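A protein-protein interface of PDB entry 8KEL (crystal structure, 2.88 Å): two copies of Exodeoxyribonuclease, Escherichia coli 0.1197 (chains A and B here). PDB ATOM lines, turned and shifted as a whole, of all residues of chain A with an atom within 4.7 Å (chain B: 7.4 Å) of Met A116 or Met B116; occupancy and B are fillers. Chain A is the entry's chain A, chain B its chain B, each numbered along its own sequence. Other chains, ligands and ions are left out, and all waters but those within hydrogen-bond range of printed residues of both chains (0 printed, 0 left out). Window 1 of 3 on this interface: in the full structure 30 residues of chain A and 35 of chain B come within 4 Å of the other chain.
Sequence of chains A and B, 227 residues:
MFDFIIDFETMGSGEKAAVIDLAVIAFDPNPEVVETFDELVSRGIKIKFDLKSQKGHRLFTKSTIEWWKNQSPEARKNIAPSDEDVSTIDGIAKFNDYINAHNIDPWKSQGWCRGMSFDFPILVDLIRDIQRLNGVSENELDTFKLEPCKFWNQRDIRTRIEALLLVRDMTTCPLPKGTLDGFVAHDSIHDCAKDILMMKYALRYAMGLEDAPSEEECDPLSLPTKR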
ATOM      1  N   CYS A 113      -6.160  12.755  18.700  1.00  0.00           N
ATOM      2  CA  CYS A 113      -5.215  13.344  19.661  1.00  0.00           C
ATOM      3  C   CYS A 113      -5.551  12.908  21.090  1.00  0.00           C
ATOM      4  O   CYS A 113      -6.517  12.180  21.333  1.00  0.00           O
ATOM      5  CB  CYS A 113      -5.179  14.863  19.562  1.00  0.00           C
ATOM      6  SG  CYS A 113      -6.740  15.639  19.889  1.00  0.00           S
ATOM      7  N   ARG A 114      -4.710  13.326  22.039  1.00  0.00           N
ATOM      8  CA  ARG A 114      -4.972  13.102  23.461  1.00  0.00           C
ATOM      9  C   ARG A 114      -5.518  14.384  24.060  1.00  0.00           C
ATOM     10  O   ARG A 114      -4.808  15.394  24.137  1.00  0.00           O
ATOM     11  CB  ARG A 114      -3.735  12.651  24.259  1.00  0.00           C
ATOM     12  CG  ARG A 114      -3.463  11.189  24.187  1.00  0.00           C
ATOM     13  CD  ARG A 114      -2.375  10.744  25.136  1.00  0.00           C
ATOM     14  NE  ARG A 114      -2.066   9.331  24.925  1.00  0.00           N
ATOM     15  CZ  ARG A 114      -2.698   8.326  25.518  1.00  0.00           C
ATOM     16  NH1 ARG A 114      -3.603   8.535  26.463  1.00  0.00           N
ATOM     17  NH2 ARG A 114      -2.422   7.075  25.147  1.00  0.00           N
ATOM     18  N   GLY A 115      -6.752  14.330  24.530  1.00  0.00           N
ATOM     19  CA  GLY A 115      -7.384  15.588  24.849  1.00  0.00           C
ATOM     20  C   GLY A 115      -7.804  16.273  23.569  1.00  0.00           C
ATOM     21  O   GLY A 115      -7.238  17.289  23.157  1.00  0.00           O
ATOM     22  N   MET A 116      -8.783  15.660  22.917  1.00  0.00           N
ATOM     23  CA  MET A 116      -9.423  16.264  21.759  1.00  0.00           C
ATOM     24  C   MET A 116      -9.769  17.744  21.966  1.00  0.00           C
ATOM     25  O   MET A 116      -9.661  18.535  21.027  1.00  0.00           O
ATOM     26  CB  MET A 116     -10.652  15.428  21.426  1.00  0.00           C
ATOM     27  CG  MET A 116     -11.435  15.834  20.247  1.00  0.00           C
ATOM     28  SD  MET A 116     -12.669  14.527  20.029  1.00  0.00           S
ATOM     29  CE  MET A 116     -13.742  15.348  18.857  1.00  0.00           C
ATOM     30  N   SER A 117     -10.129  18.151  23.184  1.00  0.00           N
ATOM     31  CA  SER A 117     -10.479  19.548  23.452  1.00  0.00           C
ATOM     32  C   SER A 117      -9.272  20.460  23.662  1.00  0.00           C
ATOM     33  O   SER A 117      -9.462  21.646  23.968  1.00  0.00           O
ATOM     34  CB  SER A 117     -11.416  19.633  24.661  1.00  0.00           C
ATOM     35  OG  SER A 117     -10.856  19.054  25.829  1.00  0.00           O
ATOM     36  N   PHE A 118      -8.053  19.948  23.513  1.00  0.00           N
ATOM     37  CA  PHE A 118      -6.832  20.735  23.614  1.00  0.00           C
ATOM     38  C   PHE A 118      -6.141  20.893  22.271  1.00  0.00           C
ATOM     39  O   PHE A 118      -5.792  22.004  21.867  1.00  0.00           O
ATOM     40  CB  PHE A 118      -5.873  20.077  24.622  1.00  0.00           C
ATOM     41  CG  PHE A 118      -4.504  20.736  24.709  1.00  0.00           C
ATOM     42  CD1 PHE A 118      -4.349  22.004  25.274  1.00  0.00           C
ATOM     43  CD2 PHE A 118      -3.360  20.056  24.265  1.00  0.00           C
ATOM     44  CE1 PHE A 118      -3.083  22.607  25.366  1.00  0.00           C
ATOM     45  CE2 PHE A 118      -2.085  20.647  24.356  1.00  0.00           C
ATOM     46  CZ  PHE A 118      -1.953  21.927  24.910  1.00  0.00           C
ATOM     47  N   ASP A 119      -5.944  19.789  21.563  1.00  0.00           N
ATOM     48  CA  ASP A 119      -5.194  19.810  20.322  1.00  0.00           C
ATOM     49  C   ASP A 119      -6.003  20.402  19.178  1.00  0.00           C
ATOM     50  O   ASP A 119      -5.536  21.326  18.508  1.00  0.00           O
ATOM     51  CB  ASP A 119      -4.735  18.395  20.000  1.00  0.00           C
ATOM     52  CG  ASP A 119      -3.498  18.007  20.757  1.00  0.00           C
ATOM     53  OD1 ASP A 119      -2.577  18.849  20.824  1.00  0.00           O
ATOM     54  OD2 ASP A 119      -3.470  16.899  21.338  1.00  0.00           O
ATOM     55  N   PHE A 120      -7.215  19.897  18.936  1.00  0.00           N
ATOM     56  CA  PHE A 120      -7.991  20.413  17.807  1.00  0.00           C
ATOM     57  C   PHE A 120      -8.385  21.883  17.932  1.00  0.00           C
ATOM     58  O   PHE A 120      -8.108  22.652  16.994  1.00  0.00           O
ATOM     59  CB  PHE A 120      -9.196  19.512  17.551  1.00  0.00           C
ATOM     60  CG  PHE A 120      -8.837  18.263  16.835  1.00  0.00           C
ATOM     61  CD1 PHE A 120      -8.459  18.316  15.494  1.00  0.00           C
ATOM     62  CD2 PHE A 120      -8.865  17.031  17.480  1.00  0.00           C
ATOM     63  CE1 PHE A 120      -8.104  17.166  14.815  1.00  0.00           C
ATOM     64  CE2 PHE A 120      -8.509  15.859  16.795  1.00  0.00           C
ATOM     65  CZ  PHE A 120      -8.128  15.931  15.468  1.00  0.00           C
ATOM     66  N   PRO A 121      -8.993  22.354  19.018  1.00  0.00           N
ATOM     67  CA  PRO A 121      -9.230  23.801  19.125  1.00  0.00           C
ATOM     68  C   PRO A 121      -8.029  24.674  18.799  1.00  0.00           C
ATOM     69  O   PRO A 121      -8.231  25.740  18.208  1.00  0.00           O
ATOM     70  CB  PRO A 121      -9.670  23.957  20.578  1.00  0.00           C
ATOM     71  CG  PRO A 121     -10.390  22.662  20.856  1.00  0.00           C
ATOM     72  CD  PRO A 121      -9.630  21.613  20.125  1.00  0.00           C
ATOM     73  N   GLN A 154     -13.388  13.751  14.017  1.00  0.00           N
ATOM     74  CA  GLN A 154     -12.418  13.862  15.077  1.00  0.00           C
ATOM     75  C   GLN A 154     -12.635  12.740  16.083  1.00  0.00           C
ATOM     76  O   GLN A 154     -13.729  12.172  16.182  1.00  0.00           O
ATOM     77  CB  GLN A 154     -12.541  15.212  15.761  1.00  0.00           C
ATOM     78  CG  GLN A 154     -12.216  16.408  14.918  1.00  0.00           C
ATOM     79  CD  GLN A 154     -12.264  17.681  15.731  1.00  0.00           C
ATOM     80  OE1 GLN A 154     -12.600  17.661  16.912  1.00  0.00           O
ATOM     81  NE2 GLN A 154     -11.904  18.788  15.120  1.00  0.00           N
ATOM     82  N   ARG A 155     -11.566  12.404  16.819  1.00  0.00           N
ATOM     83  CA  ARG A 155     -11.567  11.237  17.696  1.00  0.00           C
ATOM     84  C   ARG A 155     -10.627  11.437  18.868  1.00  0.00           C
ATOM     85  O   ARG A 155      -9.517  11.935  18.691  1.00  0.00           O
ATOM     86  CB  ARG A 155     -11.147   9.994  16.946  1.00  0.00           C
ATOM     87  CG  ARG A 155     -12.113   9.512  15.951  1.00  0.00           C
ATOM     88  CD  ARG A 155     -13.359   9.124  16.671  1.00  0.00           C
ATOM     89  NE  ARG A 155     -14.309   8.523  15.761  1.00  0.00           N
ATOM     90  CZ  ARG A 155     -15.104   9.236  14.987  1.00  0.00           C
ATOM     91  NH1 ARG A 155     -15.008  10.552  14.943  1.00  0.00           N
ATOM     92  NH2 ARG A 155     -15.999   8.614  14.226  1.00  0.00           N
ATOM     93  N   ASP A 156     -11.067  11.024  20.056  1.00  0.00           N
ATOM     94  CA  ASP A 156     -10.300  11.194  21.289  1.00  0.00           C
ATOM     95  C   ASP A 156      -9.570   9.901  21.617  1.00  0.00           C
ATOM     96  O   ASP A 156     -10.187   8.830  21.647  1.00  0.00           O
ATOM     97  CB  ASP A 156     -11.197  11.586  22.462  1.00  0.00           C
ATOM     98  CG  ASP A 156     -10.407  11.895  23.726  1.00  0.00           C
ATOM     99  OD1 ASP A 156      -9.655  12.898  23.717  1.00  0.00           O
ATOM    100  OD2 ASP A 156     -10.576  11.170  24.738  1.00  0.00           O
ATOM    101  N   GLY B 111     -16.851  13.653  32.231  1.00  0.00           N
ATOM    102  CA  GLY B 111     -17.789  14.525  31.561  1.00  0.00           C
ATOM    103  C   GLY B 111     -17.954  14.177  30.100  1.00  0.00           C
ATOM    104  O   GLY B 111     -17.083  14.457  29.280  1.00  0.00           O
ATOM    105  N   TRP B 112     -19.090  13.590  29.764  1.00  0.00           N
ATOM    106  CA  TRP B 112     -19.370  13.169  28.406  1.00  0.00           C
ATOM    107  C   TRP B 112     -19.967  14.299  27.586  1.00  0.00           C
ATOM    108  O   TRP B 112     -20.438  15.310  28.115  1.00  0.00           O
ATOM    109  CB  TRP B 112     -20.302  11.972  28.403  1.00  0.00           C
ATOM    110  CG  TRP B 112     -19.594  10.787  28.822  1.00  0.00           C
ATOM    111  CD1 TRP B 112     -19.500  10.288  30.083  1.00  0.00           C
ATOM    112  CD2 TRP B 112     -18.830   9.919  27.982  1.00  0.00           C
ATOM    113  NE1 TRP B 112     -18.726   9.148  30.079  1.00  0.00           N
ATOM    114  CE2 TRP B 112     -18.304   8.906  28.796  1.00  0.00           C
ATOM    115  CE3 TRP B 112     -18.538   9.901  26.612  1.00  0.00           C
ATOM    116  CZ2 TRP B 112     -17.509   7.887  28.287  1.00  0.00           C
ATOM    117  CZ3 TRP B 112     -17.736   8.883  26.114  1.00  0.00           C
ATOM    118  CH2 TRP B 112     -17.235   7.898  26.947  1.00  0.00           C
ATOM    119  N   CYS B 113     -19.918  14.109  26.269  1.00  0.00           N
ATOM    120  CA  CYS B 113     -20.119  15.174  25.301  1.00  0.00           C
ATOM    121  C   CYS B 113     -20.028  14.646  23.875  1.00  0.00           C
ATOM    122  O   CYS B 113     -19.223  13.765  23.597  1.00  0.00           O
ATOM    123  CB  CYS B 113     -19.094  16.256  25.561  1.00  0.00           C
ATOM    124  SG  CYS B 113     -18.923  17.391  24.276  1.00  0.00           S
ATOM    125  N   ARG B 114     -20.844  15.138  22.972  1.00  0.00           N
ATOM    126  CA  ARG B 114     -20.843  14.719  21.570  1.00  0.00           C
ATOM    127  C   ARG B 114     -20.249  15.872  20.781  1.00  0.00           C
ATOM    128  O   ARG B 114     -20.955  16.829  20.464  1.00  0.00           O
ATOM    129  CB  ARG B 114     -22.256  14.374  21.088  1.00  0.00           C
ATOM    130  CG  ARG B 114     -22.338  14.046  19.605  1.00  0.00           C
ATOM    131  CD  ARG B 114     -23.731  13.596  19.113  1.00  0.00           C
ATOM    132  NE  ARG B 114     -24.108  12.218  19.428  1.00  0.00           N
ATOM    133  CZ  ARG B 114     -23.769  11.154  18.701  1.00  0.00           C
ATOM    134  NH1 ARG B 114     -22.954  11.254  17.662  1.00  0.00           N
ATOM    135  NH2 ARG B 114     -24.266   9.960  19.023  1.00  0.00           N
ATOM    136  N   GLY B 115     -18.967  15.787  20.451  1.00  0.00           N
ATOM    137  CA  GLY B 115     -18.291  16.977  19.987  1.00  0.00           C
ATOM    138  C   GLY B 115     -17.346  17.547  21.021  1.00  0.00           C
ATOM    139  O   GLY B 115     -17.399  18.740  21.318  1.00  0.00           O
ATOM    140  N   MET B 116     -16.498  16.687  21.594  1.00  0.00           N
ATOM    141  CA  MET B 116     -15.676  17.047  22.753  1.00  0.00           C
ATOM    142  C   MET B 116     -14.833  18.308  22.544  1.00  0.00           C
ATOM    143  O   MET B 116     -14.550  19.033  23.506  1.00  0.00           O
ATOM    144  CB  MET B 116     -14.800  15.850  23.134  1.00  0.00           C
ATOM    145  CG  MET B 116     -13.853  16.077  24.284  1.00  0.00           C
ATOM    146  SD  MET B 116     -13.009  14.559  24.884  1.00  0.00           S
ATOM    147  CE  MET B 116     -11.661  15.324  25.770  1.00  0.00           C
ATOM    148  N   SER B 117     -14.423  18.596  21.311  1.00  0.00           N
ATOM    149  CA  SER B 117     -13.634  19.805  21.086  1.00  0.00           C
ATOM    150  C   SER B 117     -14.483  21.037  20.835  1.00  0.00           C
ATOM    151  O   SER B 117     -13.924  22.121  20.615  1.00  0.00           O
ATOM    152  CB  SER B 117     -12.660  19.608  19.928  1.00  0.00           C
ATOM    153  OG  SER B 117     -13.329  19.208  18.760  1.00  0.00           O
ATOM    154  N   PHE B 118     -15.808  20.901  20.887  1.00  0.00           N
ATOM    155  CA  PHE B 118     -16.747  22.007  20.777  1.00  0.00           C
ATOM    156  C   PHE B 118     -17.289  22.454  22.133  1.00  0.00           C
ATOM    157  O   PHE B 118     -17.141  23.626  22.500  1.00  0.00           O
ATOM    158  CB  PHE B 118     -17.896  21.595  19.847  1.00  0.00           C
ATOM    159  CG  PHE B 118     -18.954  22.656  19.669  1.00  0.00           C
ATOM    160  CD1 PHE B 118     -18.708  23.779  18.884  1.00  0.00           C
ATOM    161  CD2 PHE B 118     -20.186  22.542  20.299  1.00  0.00           C
ATOM    162  CE1 PHE B 118     -19.664  24.770  18.733  1.00  0.00           C
ATOM    163  CE2 PHE B 118     -21.139  23.527  20.147  1.00  0.00           C
ATOM    164  CZ  PHE B 118     -20.875  24.635  19.356  1.00  0.00           C
ATOM    165  N   ASP B 119     -17.871  21.528  22.903  1.00  0.00           N
ATOM    166  CA  ASP B 119     -18.613  21.869  24.116  1.00  0.00           C
ATOM    167  C   ASP B 119     -17.706  22.326  25.263  1.00  0.00           C
ATOM    168  O   ASP B 119     -17.810  23.466  25.742  1.00  0.00           O
ATOM    169  CB  ASP B 119     -19.440  20.662  24.528  1.00  0.00           C
ATOM    170  CG  ASP B 119     -20.701  20.534  23.732  1.00  0.00           C
ATOM    171  OD1 ASP B 119     -21.372  21.564  23.539  1.00  0.00           O
ATOM    172  OD2 ASP B 119     -21.019  19.432  23.249  1.00  0.00           O
ATOM    173  N   PHE B 120     -16.819  21.451  25.731  1.00  0.00           N
ATOM    174  CA  PHE B 120     -15.932  21.805  26.838  1.00  0.00           C
ATOM    175  C   PHE B 120     -15.127  23.084  26.625  1.00  0.00           C
ATOM    176  O   PHE B 120     -14.957  23.835  27.601  1.00  0.00           O
ATOM    177  CB  PHE B 120     -14.991  20.628  27.150  1.00  0.00           C
ATOM    178  CG  PHE B 120     -15.682  19.480  27.798  1.00  0.00           C
ATOM    179  CD1 PHE B 120     -16.122  19.592  29.110  1.00  0.00           C
ATOM    180  CD2 PHE B 120     -15.903  18.306  27.108  1.00  0.00           C
ATOM    181  CE1 PHE B 120     -16.784  18.572  29.707  1.00  0.00           C
ATOM    182  CE2 PHE B 120     -16.547  17.270  27.713  1.00  0.00           C
ATOM    183  CZ  PHE B 120     -16.993  17.402  29.014  1.00  0.00           C
ATOM    184  N   PRO B 121     -14.581  23.377  25.436  1.00  0.00           N
ATOM    185  CA  PRO B 121     -13.951  24.691  25.248  1.00  0.00           C
ATOM    186  C   PRO B 121     -14.884  25.865  25.502  1.00  0.00           C
ATOM    187  O   PRO B 121     -14.401  26.914  25.945  1.00  0.00           O
ATOM    188  CB  PRO B 121     -13.470  24.639  23.794  1.00  0.00           C
ATOM    189  CG  PRO B 121     -13.312  23.243  23.521  1.00  0.00           C
ATOM    190  CD  PRO B 121     -14.368  22.514  24.259  1.00  0.00           C
ATOM    191  N   ILE B 122     -16.191  25.735  25.224  1.00  0.00           N
ATOM    192  CA  ILE B 122     -17.131  26.791  25.599  1.00  0.00           C
ATOM    193  C   ILE B 122     -17.384  26.778  27.105  1.00  0.00           C
ATOM    194  O   ILE B 122     -17.426  27.832  27.758  1.00  0.00           O
ATOM    195  CB  ILE B 122     -18.443  26.660  24.792  1.00  0.00           C
ATOM    196  CG1 ILE B 122     -18.278  27.126  23.355  1.00  0.00           C
ATOM    197  CG2 ILE B 122     -19.571  27.455  25.403  1.00  0.00           C
ATOM    198  CD1 ILE B 122     -19.406  26.651  22.480  1.00  0.00           C
ATOM    199  N   PHE B 151      -9.364  17.515  33.130  1.00  0.00           N
ATOM    200  CA  PHE B 151      -9.393  17.576  31.670  1.00  0.00           C
ATOM    201  C   PHE B 151      -9.133  16.229  31.027  1.00  0.00           C
ATOM    202  O   PHE B 151      -9.593  16.001  29.907  1.00  0.00           O
ATOM    203  CB  PHE B 151      -8.398  18.593  31.113  1.00  0.00           C
ATOM    204  CG  PHE B 151      -6.966  18.281  31.395  1.00  0.00           C
ATOM    205  CD1 PHE B 151      -6.322  18.881  32.460  1.00  0.00           C
ATOM    206  CD2 PHE B 151      -6.251  17.396  30.581  1.00  0.00           C
ATOM    207  CE1 PHE B 151      -4.977  18.598  32.726  1.00  0.00           C
ATOM    208  CE2 PHE B 151      -4.919  17.111  30.831  1.00  0.00           C
ATOM    209  CZ  PHE B 151      -4.272  17.715  31.909  1.00  0.00           C
ATOM    210  N   TRP B 152      -8.421  15.333  31.708  1.00  0.00           N
ATOM    211  CA  TRP B 152      -8.209  13.986  31.209  1.00  0.00           C
ATOM    212  C   TRP B 152      -9.389  13.062  31.460  1.00  0.00           C
ATOM    213  O   TRP B 152      -9.352  11.918  31.001  1.00  0.00           O
ATOM    214  CB  TRP B 152      -6.971  13.389  31.848  1.00  0.00           C
ATOM    215  CG  TRP B 152      -7.065  13.330  33.339  1.00  0.00           C
ATOM    216  CD1 TRP B 152      -7.670  12.362  34.083  1.00  0.00           C
ATOM    217  CD2 TRP B 152      -6.524  14.271  34.269  1.00  0.00           C
ATOM    218  NE1 TRP B 152      -7.558  12.653  35.416  1.00  0.00           N
ATOM    219  CE2 TRP B 152      -6.845  13.813  35.560  1.00  0.00           C
ATOM    220  CE3 TRP B 152      -5.795  15.460  34.137  1.00  0.00           C
ATOM    221  CZ2 TRP B 152      -6.464  14.498  36.711  1.00  0.00           C
ATOM    222  CZ3 TRP B 152      -5.418  16.137  35.282  1.00  0.00           C
ATOM    223  CH2 TRP B 152      -5.758  15.656  36.552  1.00  0.00           C
ATOM    224  N   ASN B 153     -10.418  13.504  32.189  1.00  0.00           N
ATOM    225  CA  ASN B 153     -11.650  12.737  32.327  1.00  0.00           C
ATOM    226  C   ASN B 153     -12.754  13.208  31.396  1.00  0.00           C
ATOM    227  O   ASN B 153     -13.881  12.712  31.492  1.00  0.00           O
ATOM    228  CB  ASN B 153     -12.179  12.782  33.752  1.00  0.00           C
ATOM    229  CG  ASN B 153     -11.269  12.118  34.720  1.00  0.00           C
ATOM    230  OD1 ASN B 153     -10.774  12.758  35.644  1.00  0.00           O
ATOM    231  ND2 ASN B 153     -11.024  10.829  34.518  1.00  0.00           N
ATOM    232  N   GLN B 154     -12.467  14.172  30.527  1.00  0.00           N
ATOM    233  CA  GLN B 154     -13.394  14.512  29.467  1.00  0.00           C
ATOM    234  C   GLN B 154     -13.449  13.381  28.458  1.00  0.00           C
ATOM    235  O   GLN B 154     -12.476  12.656  28.264  1.00  0.00           O
ATOM    236  CB  GLN B 154     -12.968  15.800  28.800  1.00  0.00           C
ATOM    237  CG  GLN B 154     -13.050  16.987  29.697  1.00  0.00           C
ATOM    238  CD  GLN B 154     -12.442  18.196  29.047  1.00  0.00           C
ATOM    239  OE1 GLN B 154     -11.980  18.145  27.900  1.00  0.00           O
ATOM    240  NE2 GLN B 154     -12.380  19.286  29.795  1.00  0.00           N
ATOM    241  N   ARG B 155     -14.612  13.205  27.842  1.00  0.00           N
ATOM    242  CA  ARG B 155     -14.853  12.069  26.970  1.00  0.00           C
ATOM    243  C   ARG B 155     -15.751  12.476  25.807  1.00  0.00           C
ATOM    244  O   ARG B 155     -16.603  13.363  25.931  1.00  0.00           O
ATOM    245  CB  ARG B 155     -15.483  10.903  27.734  1.00  0.00           C
ATOM    246  CG  ARG B 155     -14.582  10.247  28.773  1.00  0.00           C
ATOM    247  CD  ARG B 155     -13.427   9.475  28.133  1.00  0.00           C
ATOM    248  NE  ARG B 155     -12.636   8.733  29.113  1.00  0.00           N
ATOM    249  CZ  ARG B 155     -11.574   9.210  29.751  1.00  0.00           C
ATOM    250  NH1 ARG B 155     -11.147  10.451  29.561  1.00  0.00           N
ATOM    251  NH2 ARG B 155     -10.929   8.424  30.608  1.00  0.00           N
ATOM    252  N   ASP B 156     -15.546  11.803  24.675  1.00  0.00           N
ATOM    253  CA  ASP B 156     -16.193  12.108  23.409  1.00  0.00           C
ATOM    254  C   ASP B 156     -17.144  10.980  23.040  1.00  0.00           C
ATOM    255  O   ASP B 156     -16.755   9.810  23.065  1.00  0.00           O
ATOM    256  CB  ASP B 156     -15.145  12.299  22.314  1.00  0.00           C
ATOM    257  CG  ASP B 156     -15.762  12.456  20.932  1.00  0.00           C
ATOM    258  OD1 ASP B 156     -16.338  13.536  20.631  1.00  0.00           O
ATOM    259  OD2 ASP B 156     -15.670  11.473  20.154  1.00  0.00           O
ATOM    260  N   ILE B 157     -18.381  11.328  22.683  1.00  0.00           N
ATOM    261  CA  ILE B 157     -19.399  10.300  22.516  1.00  0.00           C
ATOM    262  C   ILE B 157     -19.239   9.561  21.194  1.00  0.00           C
ATOM    263  O   ILE B 157     -19.380   8.334  21.140  1.00  0.00           O
ATOM    264  CB  ILE B 157     -20.796  10.912  22.690  1.00  0.00           C
ATOM    265  CG1 ILE B 157     -20.963  11.309  24.157  1.00  0.00           C
ATOM    266  CG2 ILE B 157     -21.864   9.925  22.291  1.00  0.00           C
ATOM    267  CD1 ILE B 157     -22.133  12.143  24.444  1.00  0.00           C
ATOM    268  N   ARG B 158     -18.915  10.267  20.114  1.00  0.00           N
ATOM    269  CA  ARG B 158     -18.706   9.576  18.843  1.00  0.00           C
ATOM    270  C   ARG B 158     -17.597   8.530  18.957  1.00  0.00           C
ATOM    271  O   ARG B 158     -17.772   7.380  18.538  1.00  0.00           O
ATOM    272  CB  ARG B 158     -18.372  10.570  17.733  1.00  0.00           C
ATOM    273  CG  ARG B 158     -19.416  11.561  17.408  1.00  0.00           C
ATOM    274  CD  ARG B 158     -18.906  12.388  16.279  1.00  0.00           C
ATOM    275  NE  ARG B 158     -19.808  13.481  15.948  1.00  0.00           N
ATOM    276  CZ  ARG B 158     -19.710  14.717  16.429  1.00  0.00           C
ATOM    277  NH1 ARG B 158     -18.733  15.069  17.261  1.00  0.00           N
ATOM    278  NH2 ARG B 158     -20.608  15.627  16.058  1.00  0.00           N
ATOM    279  N   THR B 159     -16.445   8.910  19.523  1.00  0.00           N
ATOM    280  CA  THR B 159     -15.361   7.945  19.730  1.00  0.00           C
ATOM    281  C   THR B 159     -15.840   6.730  20.514  1.00  0.00           C
ATOM    282  O   THR B 159     -15.570   5.583  20.137  1.00  0.00           O
ATOM    283  CB  THR B 159     -14.206   8.592  20.483  1.00  0.00           C
ATOM    284  OG1 THR B 159     -13.747   9.748  19.781  1.00  0.00           O
ATOM    285  CG2 THR B 159     -13.090   7.611  20.605  1.00  0.00           C
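OG of Ser A117 is in hydrogen-bond range of OE1 of Gln B154 (2.5 Å).
The side-chain amide oxygen (OE1) of Gln A154 lies within hydrogen-bond range of the side-chain hydroxyl (OG) of Ser B117 (2.5 Å).
The backbone NH (N) of Asp A156 sits at hydrogen-bond distance from the side-chain hydroxyl (OG1) of Thr B159 (3.0 Å).
The side-chain sulfur of Cys A113 sits close to the backbone NH of Met A116.
The backbone carbonyl oxygen of Arg A155 is in hydrogen-bond range of the backbone NH of Cys A113.
The side-chain carboxylate (OD1) of Asp A156 lies within hydrogen-bond range of the backbone NH (N) of Met A116, at 3.0 Å.
N of Met B116 is in hydrogen-bond range of OD1 of Asp B156 (3.3 Å).
The side-chain carboxylate (OD2) of Asp B156 is in hydrogen-bond range of the backbone NH (N) of Arg B158 (3.5 Å).
The side-chain hydroxyl (OG1) of Thr B159 is in hydrogen-bond range of the side-chain carboxylate (OD2) of Asp B156.
Among the printed residues, merely in contact across the chains: Met A116 with Met B116 (3.99 Å), Met A116 with Ser B117 (3.4 Å), Met A116 with Asp B156 (3.6 Å), Ser A117 with Met B116 (3.4 Å), Ser A117 with Ser B117 (3.95 Å), Pro A121 with Ser B117 (3.6 Å), Pro A121 with Pro B121 (3.997 Å), Arg A155 with Thr B159 (3.2 Å) and Asp A156 with Met B116 (3.8 Å).
No residue of chain B comes within 4 Å of Gly A115.
Printed residues of chain B within 4 Å of Met A116: Met B116 (3.99 Å), Ser B117 (3.4 Å) and Asp B156 (3.6 Å).
Printed residues of chain B within 4 Å of Ser A117: Met B116, Ser B117 and Gln B154.
Of the printed residues of chain B, Arg A155 touches Thr B159.
Of the printed residues of chain B, Asp A156 touches Met B116 and Thr B159.
Cys B113 touches none of the printed residues of chain A.
Arg B114 touches none of the printed residues of chain A.
Of the printed residues of chain A, Met B116 touches Met A116 (3.99 Å), Ser A117 (3.4 Å) and Asp A156 (3.8 Å).
Of the printed residues of chain A, Ser B117 touches Met A116 (3.4 Å), Ser A117 (3.95 Å), Pro A121 (3.6 Å) and Gln A154 (2.5 Å).
Of the printed residues of chain A, Pro B121 touches Pro A121.
Of the 12 printed residues of chain A, 6 touch a printed residue of chain B.
Printed residues of chain A that touch a printed residue of chain B: Met A116, Ser A117, Pro A121, Gln A154, Arg A155 and Asp A156.
Hydrophobic or aromatic side chains of chain A that line the printed part of chain B: Met A116 and Pro A121.
Met A116 touches Ser B117, and with the chains exchanged Ser A117 touches Met B116.
Ser A117 touches its own counterpart, Ser B117.
Ser A117 touches Gln B154, and with the chains exchanged Gln A154 touches Ser B117.
Pro B121 touches its own counterpart, Pro A121.
12 positions are printed for both chains.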
